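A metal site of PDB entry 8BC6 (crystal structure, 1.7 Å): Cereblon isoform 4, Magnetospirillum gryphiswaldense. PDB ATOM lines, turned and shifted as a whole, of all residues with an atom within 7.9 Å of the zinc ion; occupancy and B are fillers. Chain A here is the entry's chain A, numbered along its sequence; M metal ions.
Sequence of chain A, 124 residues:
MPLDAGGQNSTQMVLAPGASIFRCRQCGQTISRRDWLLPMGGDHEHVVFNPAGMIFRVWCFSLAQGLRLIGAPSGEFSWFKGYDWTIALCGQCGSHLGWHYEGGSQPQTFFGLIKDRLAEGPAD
The backbone NH (N) of Cys 24 is in hydrogen-bond range of the backbone carbonyl oxygen (O) of Gln 29 (2.8 Å).
The side-chain sulfur of Cys 27 sits close to the side-chain amide nitrogen of Gln 92.
The backbone carbonyl oxygen of Ser 95 sits at hydrogen-bond distance from the backbone NH of Cys 90 (2.8 Å).
The backbone NH of Gln 29 sits close to the side-chain sulfur of Cys 27 (3.5 Å).
The side-chain sulfur (SG) of Cys 90 lies close to the backbone NH (N) of Gln 92 (3.5 Å).
The backbone NH of Gln 26 lies close to the side-chain sulfur of Cys 24, at 3.5 Å.
The side-chain sulfur of Cys 93 lies close to the backbone NH of Ser 95 (3.4 Å).
The zinc ion is bound by the side-chain sulfur (SG) of Cys 24, the side-chain sulfur (SG) of Cys 27, the side-chain sulfur (SG) of Cys 93 and the side-chain sulfur (SG) of Cys 90.
Four residues have an atom within 4 Å of the zinc ion: Cys 24, Cys 27, Cys 90 and Cys 93.
Along chain A the residues within 4 Å of the zinc ion span positions 24 to 93.
The nearest printed residue that does not touch the zinc ion is Gln 29 (4.5 Å).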
ATOM      1  N   ARG A  23       4.664  -9.922  -1.306  1.00  0.00           N
ATOM      2  CA  ARG A  23       5.599  -9.612  -2.395  1.00  0.00           C
ATOM      3  C   ARG A  23       4.914  -8.749  -3.439  1.00  0.00           C
ATOM      4  O   ARG A  23       3.716  -8.786  -3.507  1.00  0.00           O
ATOM      5  CB  ARG A  23       6.129 -10.888  -3.049  1.00  0.00           C
ATOM      6  CG  ARG A  23       6.952 -11.748  -2.108  1.00  0.00           C
ATOM      7  CD  ARG A  23       7.491 -12.966  -2.826  1.00  0.00           C
ATOM      8  NE  ARG A  23       8.325 -13.711  -1.904  1.00  0.00           N
ATOM      9  CZ  ARG A  23       9.552 -13.330  -1.533  1.00  0.00           C
ATOM     10  NH1 ARG A  23      10.169 -12.333  -2.154  1.00  0.00           N
ATOM     11  NH2 ARG A  23      10.180 -13.980  -0.584  1.00  0.00           N
ATOM     12  N   CYS A  24       5.680  -7.969  -4.192  1.00  0.00           N
ATOM     13  CA  CYS A  24       5.194  -7.264  -5.362  1.00  0.00           C
ATOM     14  C   CYS A  24       4.558  -8.316  -6.312  1.00  0.00           C
ATOM     15  O   CYS A  24       5.237  -9.266  -6.686  1.00  0.00           O
ATOM     16  CB  CYS A  24       6.323  -6.509  -6.047  1.00  0.00           C
ATOM     17  SG  CYS A  24       5.773  -5.712  -7.574  1.00  0.00           S
ATOM     18  N   ARG A  25       3.299  -8.132  -6.682  1.00  0.00           N
ATOM     19  CA  ARG A  25       2.577  -9.049  -7.607  1.00  0.00           C
ATOM     20  C   ARG A  25       3.241  -9.075  -8.986  1.00  0.00           C
ATOM     21  O   ARG A  25       3.006 -10.051  -9.685  1.00  0.00           O
ATOM     22  CB  ARG A  25       1.121  -8.587  -7.703  1.00  0.00           C
ATOM     23  CG  ARG A  25       0.269  -9.293  -8.728  1.00  0.00           C
ATOM     24  CD  ARG A  25      -1.084  -8.630  -8.712  1.00  0.00           C
ATOM     25  NE  ARG A  25      -1.878  -9.254  -9.748  1.00  0.00           N
ATOM     26  CZ  ARG A  25      -3.156  -8.964  -9.969  1.00  0.00           C
ATOM     27  NH1 ARG A  25      -3.763  -8.046  -9.220  1.00  0.00           N
ATOM     28  NH2 ARG A  25      -3.783  -9.607 -10.928  1.00  0.00           N
ATOM     29  N   GLN A  26       3.906  -8.005  -9.417  1.00  0.00           N
ATOM     30  CA  GLN A  26       4.487  -7.894 -10.784  1.00  0.00           C
ATOM     31  C   GLN A  26       5.857  -8.577 -10.880  1.00  0.00           C
ATOM     32  O   GLN A  26       6.122  -9.127 -11.953  1.00  0.00           O
ATOM     33  CB  GLN A  26       4.513  -6.449 -11.276  1.00  0.00           C
ATOM     34  CG  GLN A  26       3.113  -5.883 -11.417  1.00  0.00           C
ATOM     35  CD  GLN A  26       2.251  -6.679 -12.354  1.00  0.00           C
ATOM     36  OE1 GLN A  26       2.721  -7.212 -13.350  1.00  0.00           O
ATOM     37  NE2 GLN A  26       0.977  -6.806 -12.018  1.00  0.00           N
ATOM     38  N   CYS A  27       6.661  -8.616  -9.820  1.00  0.00           N
ATOM     39  CA  CYS A  27       8.067  -9.097  -9.938  1.00  0.00           C
ATOM     40  C   CYS A  27       8.484 -10.006  -8.784  1.00  0.00           C
ATOM     41  O   CYS A  27       9.508 -10.636  -8.887  1.00  0.00           O
ATOM     42  CB  CYS A  27       8.961  -7.878 -10.121  1.00  0.00           C
ATOM     43  SG  CYS A  27       9.229  -6.996  -8.551  1.00  0.00           S
ATOM     44  N   GLY A  28       7.769 -10.049  -7.640  1.00  0.00           N
ATOM     45  CA  GLY A  28       8.137 -10.893  -6.504  1.00  0.00           C
ATOM     46  C   GLY A  28       9.046 -10.229  -5.477  1.00  0.00           C
ATOM     47  O   GLY A  28       9.415 -10.888  -4.471  1.00  0.00           O
ATOM     48  N   GLN A  29       9.396  -8.972  -5.646  1.00  0.00           N
ATOM     49  CA  GLN A  29      10.174  -8.258  -4.624  1.00  0.00           C
ATOM     50  C   GLN A  29       9.491  -8.408  -3.243  1.00  0.00           C
ATOM     51  O   GLN A  29       8.284  -8.144  -3.169  1.00  0.00           O
ATOM     52  CB  GLN A  29      10.274  -6.781  -4.996  1.00  0.00           C
ATOM     53  CG  GLN A  29      10.907  -5.904  -3.915  1.00  0.00           C
ATOM     54  CD  GLN A  29      12.387  -5.729  -4.059  1.00  0.00           C
ATOM     55  OE1 GLN A  29      13.133  -6.650  -4.287  1.00  0.00           O
ATOM     56  NE2 GLN A  29      12.823  -4.476  -4.023  1.00  0.00           N
ATOM     57  N   THR A  30      10.259  -8.717  -2.206  1.00  0.00           N
ATOM     58  CA  THR A  30       9.781  -8.783  -0.806  1.00  0.00           C
ATOM     59  C   THR A  30       9.367  -7.399  -0.336  1.00  0.00           C
ATOM     60  O   THR A  30      10.219  -6.483  -0.504  1.00  0.00           O
ATOM     61  CB  THR A  30      10.836  -9.351   0.159  1.00  0.00           C
ATOM     62  OG1 THR A  30      11.520 -10.452  -0.447  1.00  0.00           O
ATOM     63  CG2 THR A  30      10.142  -9.787   1.410  1.00  0.00           C
ATOM     64  N   ILE A  31       8.128  -7.208   0.162  1.00  0.00           N
ATOM     65  CA  ILE A  31       7.644  -5.847   0.522  1.00  0.00           C
ATOM     66  C   ILE A  31       7.255  -5.794   2.020  1.00  0.00           C
ATOM     67  O   ILE A  31       7.712  -4.862   2.717  1.00  0.00           O
ATOM     68  CB  ILE A  31       6.458  -5.390  -0.366  1.00  0.00           C
ATOM     69  CG1 ILE A  31       6.764  -5.385  -1.862  1.00  0.00           C
ATOM     70  CG2 ILE A  31       5.997  -4.015   0.120  1.00  0.00           C
ATOM     71  CD1 ILE A  31       7.878  -4.463  -2.286  1.00  0.00           C
ATOM     72  N   GLY A  66      11.907  -2.891   0.379  1.00  0.00           N
ATOM     73  CA  GLY A  66      12.000  -3.153  -1.060  1.00  0.00           C
ATOM     74  C   GLY A  66      11.247  -2.109  -1.870  1.00  0.00           C
ATOM     75  O   GLY A  66      11.019  -2.385  -3.076  1.00  0.00           O
ATOM     76  N   LEU A  89       6.917   3.158  -4.806  1.00  0.00           N
ATOM     77  CA  LEU A  89       7.068   2.205  -5.925  1.00  0.00           C
ATOM     78  C   LEU A  89       7.826   0.970  -5.463  1.00  0.00           C
ATOM     79  O   LEU A  89       8.630   1.043  -4.520  1.00  0.00           O
ATOM     80  CB  LEU A  89       7.859   2.850  -7.050  1.00  0.00           C
ATOM     81  CG  LEU A  89       7.379   4.191  -7.581  1.00  0.00           C
ATOM     82  CD1 LEU A  89       8.288   4.602  -8.714  1.00  0.00           C
ATOM     83  CD2 LEU A  89       5.917   4.141  -8.004  1.00  0.00           C
ATOM     84  N   CYS A  90       7.543  -0.152  -6.098  1.00  0.00           N
ATOM     85  CA  CYS A  90       8.414  -1.323  -6.026  1.00  0.00           C
ATOM     86  C   CYS A  90       9.814  -0.876  -6.404  1.00  0.00           C
ATOM     87  O   CYS A  90      10.011  -0.326  -7.494  1.00  0.00           O
ATOM     88  CB  CYS A  90       7.943  -2.409  -6.968  1.00  0.00           C
ATOM     89  SG  CYS A  90       8.963  -3.879  -6.795  1.00  0.00           S
ATOM     90  N   GLY A  91      10.784  -1.107  -5.496  1.00  0.00           N
ATOM     91  CA  GLY A  91      12.184  -0.734  -5.722  1.00  0.00           C
ATOM     92  C   GLY A  91      12.788  -1.535  -6.875  1.00  0.00           C
ATOM     93  O   GLY A  91      13.840  -1.121  -7.420  1.00  0.00           O
ATOM     94  N   GLN A  92      12.226  -2.681  -7.209  1.00  0.00           N
ATOM     95  CA  GLN A  92      12.769  -3.562  -8.256  1.00  0.00           C
ATOM     96  C   GLN A  92      12.135  -3.162  -9.614  1.00  0.00           C
ATOM     97  O   GLN A  92      12.885  -2.866 -10.561  1.00  0.00           O
ATOM     98  CB  GLN A  92      12.538  -5.005  -7.831  1.00  0.00           C
ATOM     99  CG  GLN A  92      13.077  -6.039  -8.781  1.00  0.00           C
ATOM    100  CD  GLN A  92      13.263  -7.384  -8.090  1.00  0.00           C
ATOM    101  OE1 GLN A  92      14.366  -7.730  -7.686  1.00  0.00           O
ATOM    102  NE2 GLN A  92      12.190  -8.149  -7.981  1.00  0.00           N
ATOM    103  N   CYS A  93      10.817  -3.255  -9.727  1.00  0.00           N
ATOM    104  CA  CYS A  93      10.130  -3.154 -11.029  1.00  0.00           C
ATOM    105  C   CYS A  93       9.494  -1.795 -11.274  1.00  0.00           C
ATOM    106  O   CYS A  93       9.100  -1.533 -12.435  1.00  0.00           O
ATOM    107  CB  CYS A  93       9.153  -4.289 -11.261  1.00  0.00           C
ATOM    108  SG  CYS A  93       7.565  -4.067 -10.422  1.00  0.00           S
ATOM    109  N   GLY A  94       9.335  -0.957 -10.253  1.00  0.00           N
ATOM    110  CA  GLY A  94       8.750   0.372 -10.400  1.00  0.00           C
ATOM    111  C   GLY A  94       7.225   0.349 -10.335  1.00  0.00           C
ATOM    112  O   GLY A  94       6.656   1.423 -10.454  1.00  0.00           O
ATOM    113  N   SER A  95       6.562  -0.780 -10.148  1.00  0.00           N
ATOM    114  CA  SER A  95       5.090  -0.841  -9.906  1.00  0.00           C
ATOM    115  C   SER A  95       4.684   0.118  -8.777  1.00  0.00           C
ATOM    116  O   SER A  95       5.305   0.138  -7.704  1.00  0.00           O
ATOM    117  CB  SER A  95       4.626  -2.248  -9.646  1.00  0.00           C
ATOM    118  OG  SER A  95       3.213  -2.322  -9.369  1.00  0.00           O
ATOM    119  N   HIS A  96       3.595   0.886  -8.973  1.00  0.00           N
ATOM    120  CA  HIS A  96       3.056   1.735  -7.893  1.00  0.00           C
ATOM    121  C   HIS A  96       2.351   0.849  -6.874  1.00  0.00           C
ATOM    122  O   HIS A  96       1.250   0.371  -7.167  1.00  0.00           O
ATOM    123  CB  HIS A  96       2.147   2.832  -8.463  1.00  0.00           C
ATOM    124  CG  HIS A  96       1.554   3.630  -7.374  1.00  0.00           C
ATOM    125  ND1 HIS A  96       0.348   4.332  -7.514  1.00  0.00           N
ATOM    126  CD2 HIS A  96       2.044   3.928  -6.135  1.00  0.00           C
ATOM    127  CE1 HIS A  96       0.145   5.012  -6.407  1.00  0.00           C
ATOM    128  NE2 HIS A  96       1.160   4.741  -5.537  1.00  0.00           N
ATOM    129  N   LEU A  97       2.954   0.643  -5.696  1.00  0.00           N
ATOM    130  CA  LEU A  97       2.410  -0.247  -4.666  1.00  0.00           C
ATOM    131  C   LEU A  97       1.596   0.496  -3.612  1.00  0.00           C
ATOM    132  O   LEU A  97       0.821  -0.147  -2.924  1.00  0.00           O
ATOM    133  CB  LEU A  97       3.534  -1.066  -4.063  1.00  0.00           C
ATOM    134  CG  LEU A  97       4.240  -2.041  -5.007  1.00  0.00           C
ATOM    135  CD1 LEU A  97       5.217  -2.920  -4.236  1.00  0.00           C
ATOM    136  CD2 LEU A  97       3.260  -2.914  -5.771  1.00  0.00           C
ATOM    137  N   ARG A 117      -2.123  -5.214  -5.435  1.00  0.00           N
ATOM    138  CA  ARG A 117      -0.827  -5.092  -6.119  1.00  0.00           C
ATOM    139  C   ARG A 117       0.240  -5.940  -5.423  1.00  0.00           C
ATOM    140  O   ARG A 117       1.447  -5.878  -5.836  1.00  0.00           O
ATOM    141  CB  ARG A 117      -0.497  -3.621  -6.220  1.00  0.00           C
ATOM    142  CG  ARG A 117      -1.505  -2.938  -7.121  1.00  0.00           C
ATOM    143  CD  ARG A 117      -1.140  -1.556  -7.520  1.00  0.00           C
ATOM    144  NE  ARG A 117      -2.278  -0.946  -8.206  1.00  0.00           N
ATOM    145  CZ  ARG A 117      -2.240   0.282  -8.760  1.00  0.00           C
ATOM    146  NH1 ARG A 117      -1.107   0.975  -8.754  1.00  0.00           N
ATOM    147  NH2 ARG A 117      -3.331   0.789  -9.345  1.00  0.00           N
HETATM  148 ZN    ZN M   1       7.821  -5.183  -8.409  1.00  0.00          ZN
